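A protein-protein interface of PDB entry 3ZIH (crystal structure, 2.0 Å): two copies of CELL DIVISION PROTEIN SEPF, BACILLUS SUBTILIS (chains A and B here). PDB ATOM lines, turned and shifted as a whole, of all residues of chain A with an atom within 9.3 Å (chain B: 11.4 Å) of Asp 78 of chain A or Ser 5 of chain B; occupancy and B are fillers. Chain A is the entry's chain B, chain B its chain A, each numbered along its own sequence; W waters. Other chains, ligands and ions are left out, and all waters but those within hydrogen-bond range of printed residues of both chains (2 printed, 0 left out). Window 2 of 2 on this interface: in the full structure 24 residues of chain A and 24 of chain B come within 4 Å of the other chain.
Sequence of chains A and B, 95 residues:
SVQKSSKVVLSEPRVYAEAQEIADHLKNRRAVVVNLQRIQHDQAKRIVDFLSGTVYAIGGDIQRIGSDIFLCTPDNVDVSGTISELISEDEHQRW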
ATOM      1  N   SER A   5     -32.133  20.723   7.571  1.00  0.00           N
ATOM      2  CA  SER A   5     -30.864  19.902   7.573  1.00  0.00           C
ATOM      3  C   SER A   5     -29.871  20.205   8.759  1.00  0.00           C
ATOM      4  O   SER A   5     -29.682  19.323   9.599  1.00  0.00           O
ATOM      5  CB  SER A   5     -30.165  19.986   6.227  1.00  0.00           C
ATOM      6  OG  SER A   5     -29.001  19.185   6.208  1.00  0.00           O
ATOM      7  N   SER A   6     -29.240  21.384   8.861  1.00  0.00           N
ATOM      8  CA  SER A   6     -28.616  21.724  10.150  1.00  0.00           C
ATOM      9  C   SER A   6     -29.673  22.372  11.062  1.00  0.00           C
ATOM     10  O   SER A   6     -30.695  22.793  10.583  1.00  0.00           O
ATOM     11  CB  SER A   6     -27.339  22.556  10.005  1.00  0.00           C
ATOM     12  OG  SER A   6     -27.509  23.842   9.408  1.00  0.00           O
ATOM     13  N   ARG A  29     -24.375  18.366  19.053  1.00  0.00           N
ATOM     14  CA  ARG A  29     -23.964  18.979  17.794  1.00  0.00           C
ATOM     15  C   ARG A  29     -24.893  20.037  17.243  1.00  0.00           C
ATOM     16  O   ARG A  29     -24.878  20.289  16.050  1.00  0.00           O
ATOM     17  CB  ARG A  29     -23.664  17.912  16.715  1.00  0.00           C
ATOM     18  CG  ARG A  29     -22.542  17.012  17.201  1.00  0.00           C
ATOM     19  CD  ARG A  29     -21.530  16.603  16.096  1.00  0.00           C
ATOM     20  NE  ARG A  29     -20.346  16.037  16.751  1.00  0.00           N
ATOM     21  CZ  ARG A  29     -19.427  16.742  17.411  1.00  0.00           C
ATOM     22  NH1 ARG A  29     -19.509  18.074  17.488  1.00  0.00           N
ATOM     23  NH2 ARG A  29     -18.428  16.104  18.025  1.00  0.00           N
ATOM     24  N   ALA A  31     -25.897  24.243  17.213  1.00  0.00           N
ATOM     25  CA  ALA A  31     -25.607  25.619  17.617  1.00  0.00           C
ATOM     26  C   ALA A  31     -26.777  26.176  18.382  1.00  0.00           C
ATOM     27  O   ALA A  31     -27.976  25.797  18.154  1.00  0.00           O
ATOM     28  CB  ALA A  31     -25.315  26.498  16.388  1.00  0.00           C
ATOM     29  N   GLY A  59     -14.655  21.300  22.568  1.00  0.00           N
ATOM     30  CA  GLY A  59     -13.979  21.820  21.407  1.00  0.00           C
ATOM     31  C   GLY A  59     -14.897  22.714  20.578  1.00  0.00           C
ATOM     32  O   GLY A  59     -14.738  22.813  19.379  1.00  0.00           O
ATOM     33  N   GLY A  60     -15.853  23.384  21.200  1.00  0.00           N
ATOM     34  CA  GLY A  60     -16.704  24.300  20.453  1.00  0.00           C
ATOM     35  C   GLY A  60     -16.293  25.736  20.626  1.00  0.00           C
ATOM     36  O   GLY A  60     -15.137  26.009  20.885  1.00  0.00           O
ATOM     37  N   ASP A  61     -17.215  26.686  20.452  1.00  0.00           N
ATOM     38  CA  ASP A  61     -16.860  28.075  20.688  1.00  0.00           C
ATOM     39  C   ASP A  61     -18.048  28.814  21.235  1.00  0.00           C
ATOM     40  O   ASP A  61     -19.229  28.366  21.111  1.00  0.00           O
ATOM     41  CB  ASP A  61     -16.350  28.705  19.396  1.00  0.00           C
ATOM     42  CG  ASP A  61     -15.436  29.931  19.632  1.00  0.00           C
ATOM     43  OD1 ASP A  61     -15.023  30.264  20.814  1.00  0.00           O
ATOM     44  OD2 ASP A  61     -15.119  30.596  18.623  1.00  0.00           O
ATOM     45  N   GLN A  63     -19.292  32.996  21.364  1.00  0.00           N
ATOM     46  CA  GLN A  63     -18.908  34.299  20.789  1.00  0.00           C
ATOM     47  C   GLN A  63     -20.045  35.289  21.043  1.00  0.00           C
ATOM     48  O   GLN A  63     -21.205  34.931  20.865  1.00  0.00           O
ATOM     49  CB  GLN A  63     -18.640  34.039  19.312  1.00  0.00           C
ATOM     50  CG  GLN A  63     -18.120  35.133  18.573  1.00  0.00           C
ATOM     51  CD  GLN A  63     -17.671  34.720  17.139  1.00  0.00           C
ATOM     52  OE1 GLN A  63     -17.596  33.543  16.768  1.00  0.00           O
ATOM     53  NE2 GLN A  63     -17.357  35.718  16.363  1.00  0.00           N
ATOM     54  N   LEU A  71     -23.585  33.356  20.628  1.00  0.00           N
ATOM     55  CA  LEU A  71     -23.743  32.172  19.823  1.00  0.00           C
ATOM     56  C   LEU A  71     -22.742  31.124  20.358  1.00  0.00           C
ATOM     57  O   LEU A  71     -21.519  31.396  20.387  1.00  0.00           O
ATOM     58  CB  LEU A  71     -23.427  32.489  18.369  1.00  0.00           C
ATOM     59  CG  LEU A  71     -23.388  31.274  17.399  1.00  0.00           C
ATOM     60  CD1 LEU A  71     -24.785  30.677  17.302  1.00  0.00           C
ATOM     61  CD2 LEU A  71     -22.872  31.782  16.019  1.00  0.00           C
ATOM     62  N   THR A  73     -21.367  27.350  19.619  1.00  0.00           N
ATOM     63  CA  THR A  73     -21.293  26.370  18.572  1.00  0.00           C
ATOM     64  C   THR A  73     -20.513  25.131  18.999  1.00  0.00           C
ATOM     65  O   THR A  73     -19.572  25.242  19.776  1.00  0.00           O
ATOM     66  CB  THR A  73     -20.615  26.944  17.349  1.00  0.00           C
ATOM     67  OG1 THR A  73     -19.468  27.713  17.744  1.00  0.00           O
ATOM     68  CG2 THR A  73     -21.601  27.876  16.644  1.00  0.00           C
ATOM     69  N   PRO A  74     -20.941  23.955  18.541  1.00  0.00           N
ATOM     70  CA  PRO A  74     -20.132  22.754  18.661  1.00  0.00           C
ATOM     71  C   PRO A  74     -19.006  22.812  17.627  1.00  0.00           C
ATOM     72  O   PRO A  74     -18.982  23.755  16.780  1.00  0.00           O
ATOM     73  CB  PRO A  74     -21.121  21.641  18.292  1.00  0.00           C
ATOM     74  CG  PRO A  74     -22.024  22.280  17.275  1.00  0.00           C
ATOM     75  CD  PRO A  74     -22.091  23.752  17.614  1.00  0.00           C
ATOM     76  N   ASP A  75     -18.115  21.800  17.635  1.00  0.00           N
ATOM     77  CA  ASP A  75     -16.961  21.802  16.693  1.00  0.00           C
ATOM     78  C   ASP A  75     -17.339  21.611  15.219  1.00  0.00           C
ATOM     79  O   ASP A  75     -16.560  21.899  14.331  1.00  0.00           O
ATOM     80  CB  ASP A  75     -15.810  20.842  17.121  1.00  0.00           C
ATOM     81  CG  ASP A  75     -16.171  19.344  17.007  1.00  0.00           C
ATOM     82  OD1 ASP A  75     -17.293  18.973  16.627  1.00  0.00           O
ATOM     83  OD2 ASP A  75     -15.277  18.515  17.288  1.00  0.00           O
ATOM     84  N   ASN A  76     -18.540  21.158  14.955  1.00  0.00           N
ATOM     85  CA  ASN A  76     -18.987  20.944  13.589  1.00  0.00           C
ATOM     86  C   ASN A  76     -19.674  22.203  12.953  1.00  0.00           C
ATOM     87  O   ASN A  76     -20.286  22.091  11.855  1.00  0.00           O
ATOM     88  CB  ASN A  76     -19.963  19.758  13.534  1.00  0.00           C
ATOM     89  CG  ASN A  76     -21.163  19.906  14.484  1.00  0.00           C
ATOM     90  OD1 ASN A  76     -21.001  19.714  15.663  1.00  0.00           O
ATOM     91  ND2 ASN A  76     -22.385  20.177  13.959  1.00  0.00           N
ATOM     92  N   VAL A  77     -19.611  23.357  13.635  1.00  0.00           N
ATOM     93  CA  VAL A  77     -20.154  24.607  13.077  1.00  0.00           C
ATOM     94  C   VAL A  77     -19.065  25.633  12.988  1.00  0.00           C
ATOM     95  O   VAL A  77     -18.606  26.108  14.011  1.00  0.00           O
ATOM     96  CB  VAL A  77     -21.368  25.170  13.872  1.00  0.00           C
ATOM     97  CG1 VAL A  77     -21.754  26.630  13.369  1.00  0.00           C
ATOM     98  CG2 VAL A  77     -22.617  24.188  13.747  1.00  0.00           C
ATOM     99  N   ASP A  78     -18.646  26.007  11.766  1.00  0.00           N
ATOM    100  CA  ASP A  78     -17.708  27.136  11.623  1.00  0.00           C
ATOM    101  C   ASP A  78     -18.406  28.481  11.539  1.00  0.00           C
ATOM    102  O   ASP A  78     -19.328  28.648  10.720  1.00  0.00           O
ATOM    103  CB  ASP A  78     -16.898  27.008  10.361  1.00  0.00           C
ATOM    104  CG  ASP A  78     -16.082  25.733  10.328  1.00  0.00           C
ATOM    105  OD1 ASP A  78     -15.515  25.384  11.401  1.00  0.00           O
ATOM    106  OD2 ASP A  78     -16.046  25.095   9.232  1.00  0.00           O
ATOM    107  N   VAL A  79     -17.935  29.452  12.325  1.00  0.00           N
ATOM    108  CA  VAL A  79     -18.510  30.782  12.349  1.00  0.00           C
ATOM    109  C   VAL A  79     -17.553  31.713  11.638  1.00  0.00           C
ATOM    110  O   VAL A  79     -16.345  31.713  11.958  1.00  0.00           O
ATOM    111  CB  VAL A  79     -18.688  31.271  13.792  1.00  0.00           C
ATOM    112  CG1 VAL A  79     -19.363  32.718  13.827  1.00  0.00           C
ATOM    113  CG2 VAL A  79     -19.493  30.254  14.544  1.00  0.00           C
ATOM    114  N   SER A  80     -18.039  32.503  10.681  1.00  0.00           N
ATOM    115  CA  SER A  80     -17.196  33.525  10.057  1.00  0.00           C
ATOM    116  C   SER A  80     -17.797  34.920  10.188  1.00  0.00           C
ATOM    117  O   SER A  80     -19.025  35.097  10.190  1.00  0.00           O
ATOM    118  CB  SER A  80     -16.980  33.199   8.583  1.00  0.00           C
ATOM    119  OG  SER A  80     -18.213  33.188   7.926  1.00  0.00           O
ATOM    120  N   GLY A  81     -16.917  35.906  10.282  1.00  0.00           N
ATOM    121  CA  GLY A  81     -17.297  37.293  10.431  1.00  0.00           C
ATOM    122  C   GLY A  81     -17.151  37.710  11.881  1.00  0.00           C
ATOM    123  O   GLY A  81     -16.918  36.877  12.764  1.00  0.00           O
ATOM    124  N   SER B   5     -20.324  19.315   8.467  1.00  0.00           N
ATOM    125  CA  SER B   5     -19.978  20.655   8.974  1.00  0.00           C
ATOM    126  C   SER B   5     -20.975  21.687   8.384  1.00  0.00           C
ATOM    127  O   SER B   5     -21.561  21.445   7.309  1.00  0.00           O
ATOM    128  CB  SER B   5     -18.517  20.992   8.629  1.00  0.00           C
ATOM    129  OG  SER B   5     -18.020  22.146   9.348  1.00  0.00           O
ATOM    130  N   SER B   6     -21.212  22.784   9.122  1.00  0.00           N
ATOM    131  CA  SER B   6     -22.023  23.927   8.624  1.00  0.00           C
ATOM    132  C   SER B   6     -21.316  25.268   8.908  1.00  0.00           C
ATOM    133  O   SER B   6     -20.362  25.313   9.690  1.00  0.00           O
ATOM    134  CB  SER B   6     -23.473  23.880   9.161  1.00  0.00           C
ATOM    135  OG  SER B   6     -23.587  24.124  10.571  1.00  0.00           O
ATOM    136  N   LYS B   7     -21.744  26.328   8.203  1.00  0.00           N
ATOM    137  CA  LYS B   7     -21.171  27.645   8.359  1.00  0.00           C
ATOM    138  C   LYS B   7     -22.279  28.671   8.688  1.00  0.00           C
ATOM    139  O   LYS B   7     -23.338  28.713   8.045  1.00  0.00           O
ATOM    140  CB  LYS B   7     -20.387  28.123   7.108  1.00  0.00           C
ATOM    141  CG  LYS B   7     -19.738  27.008   6.276  1.00  0.00           C
ATOM    142  CD  LYS B   7     -18.871  27.551   5.113  1.00  0.00           C
ATOM    143  CE  LYS B   7     -17.669  26.627   4.842  1.00  0.00           C
ATOM    144  NZ  LYS B   7     -16.761  27.145   3.769  1.00  0.00           N
ATOM    145  N   VAL B   8     -22.013  29.479   9.700  1.00  0.00           N
ATOM    146  CA  VAL B   8     -22.887  30.552  10.118  1.00  0.00           C
ATOM    147  C   VAL B   8     -22.106  31.843   9.934  1.00  0.00           C
ATOM    148  O   VAL B   8     -20.916  31.916  10.358  1.00  0.00           O
ATOM    149  CB  VAL B   8     -23.241  30.414  11.595  1.00  0.00           C
ATOM    150  CG1 VAL B   8     -24.104  31.602  12.018  1.00  0.00           C
ATOM    151  CG2 VAL B   8     -23.927  29.057  11.862  1.00  0.00           C
ATOM    152  N   VAL B   9     -22.734  32.855   9.332  1.00  0.00           N
ATOM    153  CA  VAL B   9     -22.054  34.094   9.076  1.00  0.00           C
ATOM    154  C   VAL B   9     -22.565  35.121  10.084  1.00  0.00           C
ATOM    155  O   VAL B   9     -23.746  35.079  10.428  1.00  0.00           O
ATOM    156  CB  VAL B   9     -22.266  34.550   7.612  1.00  0.00           C
ATOM    157  CG1 VAL B   9     -21.576  35.937   7.343  1.00  0.00           C
ATOM    158  CG2 VAL B   9     -21.696  33.472   6.644  1.00  0.00           C
ATOM    159  N   LEU B  10     -21.665  35.927  10.637  1.00  0.00           N
ATOM    160  CA  LEU B  10     -22.007  37.046  11.504  1.00  0.00           C
ATOM    161  C   LEU B  10     -21.824  38.341  10.677  1.00  0.00           C
ATOM    162  O   LEU B  10     -20.770  38.572  10.087  1.00  0.00           O
ATOM    163  CB  LEU B  10     -21.138  37.147  12.735  1.00  0.00           C
ATOM    164  CG  LEU B  10     -20.840  35.855  13.473  1.00  0.00           C
ATOM    165  CD1 LEU B  10     -19.930  36.214  14.658  1.00  0.00           C
ATOM    166  CD2 LEU B  10     -22.148  35.210  13.914  1.00  0.00           C
ATOM    167  N   SER B  11     -22.842  39.180  10.675  1.00  0.00           N
ATOM    168  CA  SER B  11     -22.832  40.408   9.881  1.00  0.00           C
ATOM    169  C   SER B  11     -23.295  41.555  10.766  1.00  0.00           C
ATOM    170  O   SER B  11     -24.178  41.362  11.579  1.00  0.00           O
ATOM    171  CB  SER B  11     -23.819  40.222   8.728  1.00  0.00           C
ATOM    172  OG  SER B  11     -23.906  41.392   7.956  1.00  0.00           O
ATOM    173  N   HIS B  25     -25.290  35.267   0.949  1.00  0.00           N
ATOM    174  CA  HIS B  25     -24.990  34.182   1.879  1.00  0.00           C
ATOM    175  C   HIS B  25     -26.189  33.223   1.972  1.00  0.00           C
ATOM    176  O   HIS B  25     -26.019  31.990   2.003  1.00  0.00           O
ATOM    177  CB  HIS B  25     -24.609  34.718   3.253  1.00  0.00           C
ATOM    178  CG  HIS B  25     -23.180  35.155   3.347  1.00  0.00           C
ATOM    179  ND1 HIS B  25     -22.132  34.291   3.046  1.00  0.00           N
ATOM    180  CD2 HIS B  25     -22.614  36.342   3.690  1.00  0.00           C
ATOM    181  CE1 HIS B  25     -20.985  34.940   3.236  1.00  0.00           C
ATOM    182  NE2 HIS B  25     -21.255  36.185   3.598  1.00  0.00           N
ATOM    183  N   ASN B  28     -26.662  31.030  -0.928  1.00  0.00           N
ATOM    184  CA  ASN B  28     -25.640  30.020  -0.804  1.00  0.00           C
ATOM    185  C   ASN B  28     -25.777  29.085   0.423  1.00  0.00           C
ATOM    186  O   ASN B  28     -24.781  28.525   0.875  1.00  0.00           O
ATOM    187  CB  ASN B  28     -24.288  30.732  -0.774  1.00  0.00           C
ATOM    188  CG  ASN B  28     -23.930  31.367  -2.139  1.00  0.00           C
ATOM    189  OD1 ASN B  28     -24.360  30.902  -3.150  1.00  0.00           O
ATOM    190  ND2 ASN B  28     -23.156  32.408  -2.119  1.00  0.00           N
ATOM    191  N   ARG B  29     -26.984  29.022   1.011  1.00  0.00           N
ATOM    192  CA  ARG B  29     -27.335  28.038   2.022  1.00  0.00           C
ATOM    193  C   ARG B  29     -26.701  28.212   3.393  1.00  0.00           C
ATOM    194  O   ARG B  29     -26.630  27.242   4.138  1.00  0.00           O
ATOM    195  CB  ARG B  29     -27.082  26.587   1.479  1.00  0.00           C
ATOM    196  CG  ARG B  29     -27.942  26.350   0.257  1.00  0.00           C
ATOM    197  CD  ARG B  29     -27.917  24.946  -0.260  1.00  0.00           C
ATOM    198  NE  ARG B  29     -28.341  25.118  -1.624  1.00  0.00           N
ATOM    199  CZ  ARG B  29     -29.611  25.119  -2.024  1.00  0.00           C
ATOM    200  NH1 ARG B  29     -30.598  24.882  -1.157  1.00  0.00           N
ATOM    201  NH2 ARG B  29     -29.876  25.324  -3.314  1.00  0.00           N
ATOM    202  N   ARG B  30     -26.218  29.424   3.705  1.00  0.00           N
ATOM    203  CA  ARG B  30     -25.708  29.738   5.027  1.00  0.00           C
ATOM    204  C   ARG B  30     -26.703  30.624   5.835  1.00  0.00           C
ATOM    205  O   ARG B  30     -27.277  31.581   5.317  1.00  0.00           O
ATOM    206  CB  ARG B  30     -24.331  30.414   4.959  1.00  0.00           C
ATOM    207  CG  ARG B  30     -23.254  29.573   4.199  1.00  0.00           C
ATOM    208  CD  ARG B  30     -21.910  30.208   4.114  1.00  0.00           C
ATOM    209  NE  ARG B  30     -21.811  31.169   3.028  1.00  0.00           N
ATOM    210  CZ  ARG B  30     -21.519  30.931   1.742  1.00  0.00           C
ATOM    211  NH1 ARG B  30     -21.259  29.709   1.303  1.00  0.00           N
ATOM    212  NH2 ARG B  30     -21.485  31.967   0.880  1.00  0.00           N
ATOM    213  N   ALA B  31     -26.863  30.270   7.113  1.00  0.00           N
ATOM    214  CA  ALA B  31     -27.502  31.134   8.110  1.00  0.00           C
ATOM    215  C   ALA B  31     -26.677  32.389   8.293  1.00  0.00           C
ATOM    216  O   ALA B  31     -25.448  32.350   8.214  1.00  0.00           O
ATOM    217  CB  ALA B  31     -27.591  30.373   9.447  1.00  0.00           C
ATOM    218  N   VAL B  32     -27.317  33.516   8.589  1.00  0.00           N
ATOM    219  CA  VAL B  32     -26.575  34.729   8.901  1.00  0.00           C
ATOM    220  C   VAL B  32     -27.228  35.364  10.143  1.00  0.00           C
ATOM    221  O   VAL B  32     -28.476  35.562  10.211  1.00  0.00           O
ATOM    222  CB  VAL B  32     -26.681  35.774   7.744  1.00  0.00           C
ATOM    223  CG1 VAL B  32     -25.862  36.987   8.081  1.00  0.00           C
ATOM    224  CG2 VAL B  32     -26.299  35.133   6.377  1.00  0.00           C
ATOM    225  N   VAL B  33     -26.375  35.752  11.065  1.00  0.00           N
ATOM    226  CA  VAL B  33     -26.801  36.556  12.204  1.00  0.00           C
ATOM    227  C   VAL B  33     -26.603  37.988  11.786  1.00  0.00           C
ATOM    228  O   VAL B  33     -25.484  38.354  11.389  1.00  0.00           O
ATOM    229  CB  VAL B  33     -25.931  36.245  13.477  1.00  0.00           C
ATOM    230  CG1 VAL B  33     -26.259  37.247  14.626  1.00  0.00           C
ATOM    231  CG2 VAL B  33     -26.214  34.836  13.947  1.00  0.00           C
ATOM    232  N   LEU B  71     -31.861  36.609  13.040  1.00  0.00           N
ATOM    233  CA  LEU B  71     -31.312  35.401  12.496  1.00  0.00           C
ATOM    234  C   LEU B  71     -32.024  35.162  11.168  1.00  0.00           C
ATOM    235  O   LEU B  71     -33.246  35.011  11.133  1.00  0.00           O
ATOM    236  CB  LEU B  71     -31.525  34.212  13.444  1.00  0.00           C
ATOM    237  CG  LEU B  71     -30.994  32.859  12.861  1.00  0.00           C
ATOM    238  CD1 LEU B  71     -29.451  32.892  12.527  1.00  0.00           C
ATOM    239  CD2 LEU B  71     -31.394  31.706  13.782  1.00  0.00           C
ATOM    240  N   ASN B  76     -32.595  25.191   4.412  1.00  0.00           N
ATOM    241  CA  ASN B  76     -31.853  24.018   4.883  1.00  0.00           C
ATOM    242  C   ASN B  76     -31.401  24.144   6.337  1.00  0.00           C
ATOM    243  O   ASN B  76     -30.718  23.247   6.834  1.00  0.00           O
ATOM    244  CB  ASN B  76     -30.598  23.728   3.998  1.00  0.00           C
ATOM    245  CG  ASN B  76     -29.717  24.942   3.833  1.00  0.00           C
ATOM    246  OD1 ASN B  76     -30.091  25.897   3.132  1.00  0.00           O
ATOM    247  ND2 ASN B  76     -28.596  24.959   4.522  1.00  0.00           N
ATOM    248  N   VAL B  77     -31.756  25.259   7.008  1.00  0.00           N
ATOM    249  CA  VAL B  77     -31.472  25.429   8.448  1.00  0.00           C
ATOM    250  C   VAL B  77     -32.799  25.450   9.187  1.00  0.00           C
ATOM    251  O   VAL B  77     -33.682  26.284   8.916  1.00  0.00           O
ATOM    252  CB  VAL B  77     -30.635  26.683   8.740  1.00  0.00           C
ATOM    253  CG1 VAL B  77     -30.393  26.831  10.187  1.00  0.00           C
ATOM    254  CG2 VAL B  77     -29.309  26.643   7.974  1.00  0.00           C
HETATM  255  O   HOH W   1     -27.019  23.615   6.944  1.00  0.00           O
HETATM  256  O   HOH W   2     -26.086  26.202  10.503  1.00  0.00           O
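Hydrophobic or aromatic side chains of chain A within 4 Å of the printed part of chain B: Val 77 and Val 79.
Of the 17 printed residues of chain B, 8 touch a printed residue of chain A.
Among the printed residues, 18 pairs touch across the chains.
Among the printed residues, no Asp or Glu carboxylate lies within 4 Å of a Lys or Arg side-chain nitrogen of the other chain.
Water W1 bridges the side-chain hydroxyl (OG) of Ser 6 of chain A and the side-chain amide nitrogen (ND2) of Asn 76 of chain B.
Water W2 bridges the side-chain hydroxyl of Ser 6 of chain A and the side-chain hydroxyl of Ser 6 of chain B.
N of Val 9 of chain B lies within hydrogen-bond range of O of Ala 31 of chain B (3.0 Å).
N of Val 33 of chain B sits at hydrogen-bond distance from O of Val 9 of chain B (2.8 Å).
The side-chain amide nitrogen (ND2) of Asn 76 of chain B lies within hydrogen-bond range of the backbone carbonyl oxygen (O) of Arg 29 of chain B (3.0 Å).
The side-chain amide oxygen of Asn 76 of chain A sits at hydrogen-bond distance from the guanidinium group of Arg 29 of chain A, 2.9 Å away.
O of Gln 63 of chain A is in hydrogen-bond range of N of Leu 71 of chain A (2.9 Å).
OG of Ser 5 of chain B sits close to O of Asn 76 of chain A.
The backbone carbonyl oxygen (O) of Asn 76 of chain A sits at hydrogen-bond distance from the backbone NH (N) of Ser 6 of chain B (3.0 Å).
O of Ser 6 of chain B lies within hydrogen-bond range of N of Asp 78 of chain A (2.8 Å).
N of Val 8 of chain B lies within hydrogen-bond range of O of Asp 78 of chain A, 3.0 Å away.
O of Val 8 of chain B sits at hydrogen-bond distance from N of Ser 80 of chain A (3.0 Å).
The backbone NH (N) of Leu 10 of chain B lies within hydrogen-bond range of the backbone carbonyl oxygen (O) of Ser 80 of chain A.
The backbone carbonyl oxygen (O) of Asn 76 of chain B lies within hydrogen-bond range of the backbone NH (N) of Ser 5 of chain A.
The backbone carbonyl oxygen of Asn 76 of chain B is in hydrogen-bond range of the backbone NH of Ser 6 of chain A (3.1 Å).
Ser 5 of chain A touches Asn 76 of chain B, and with the chains exchanged Asn 76 of chain A touches Ser 5 of chain B.
Ser 6 of chain A touches Asn 76 of chain B, and with the chains exchanged Asn 76 of chain A touches Ser 6 of chain B.
Ser 6 of chain A touches Val 77 of chain B, and with the chains exchanged Val 77 of chain A touches Ser 6 of chain B.
Asp 78 of chain A touches just these residues of chain B: Ser 5 (3.6 Å), Ser 6 (2.8 Å), Lys 7 (3.2 Å) and Val 8 (3.0 Å).
Ser 5 of chain B touches two residues of chain A.
Of chain B, only Ser 5 and Ser 6 come within 4 Å of Asn 76 of chain A.
Val 77 of chain A touches two residues of chain B.
Val 79 of chain A touches two residues of chain B.
Of chain B, only Val 8 (3.0 Å), Val 9 (3.4 Å) and Leu 10 (2.8 Å) come within 4 Å of Ser 80 of chain A.
Of the printed residues of chain A, Ser 6 of chain B touches Asn 76 (3.0 Å), Val 77 (3.3 Å) and Asp 78 (2.8 Å).
Of the printed residues of chain A, Leu 10 of chain B touches Gln 63, Val 79, Ser 80 and Gly 81.
Printed residues of chain A within 4 Å of Val 77 of chain B: Ser 6 (3.5 Å).
Printed residues of chain A within 4 Å of Val 8 of chain B: Val 77 (3.6 Å), Asp 78 (3.0 Å), Val 79 (3.3 Å) and Ser 80 (3.0 Å).
Of the printed residues of chain A, Asn 76 of chain B touches Ser 5 (3.0 Å) and Ser 6 (3.1 Å).
Of the printed residues of chain B, Gln 63 of chain A touches Leu 10 (3.1 Å).
The nearest residue of chain B that does not touch Asp 78 of chain A is Val 9 of chain B (5.6 Å).
The nearest residue of chain A that does not touch Ser 5 of chain B is Val 77 of chain A (4.7 Å).
Ser 6 of chain A touches Val 77 of chain B.
Gln 63 of chain A touches Leu 10 of chain B (NE2 to CD1, 3.1 Å).
Ser 6 of chain B touches Val 77 of chain A (OG to CG2, 3.3 Å).
CG1 of Val 77 of chain A touches CG2 of Val 8 of chain B, at 3.6 Å.
Asp 78 of chain A touches Ser 5 of chain B (OD2 to OG, 3.6 Å).
Lys 7 of chain B touches Asp 78 of chain A.
Val 8 of chain B touches Val 79 of chain A (O to CA, 3.3 Å).
Leu 10 of chain B touches Val 79 of chain A (CG to CG1, 3.5 Å).
Ser 80 of chain A touches Val 9 of chain B (O to CA, 3.4 Å).
O of Gly 81 of chain A touches CD1 of Leu 10 of chain B (3.6 Å).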
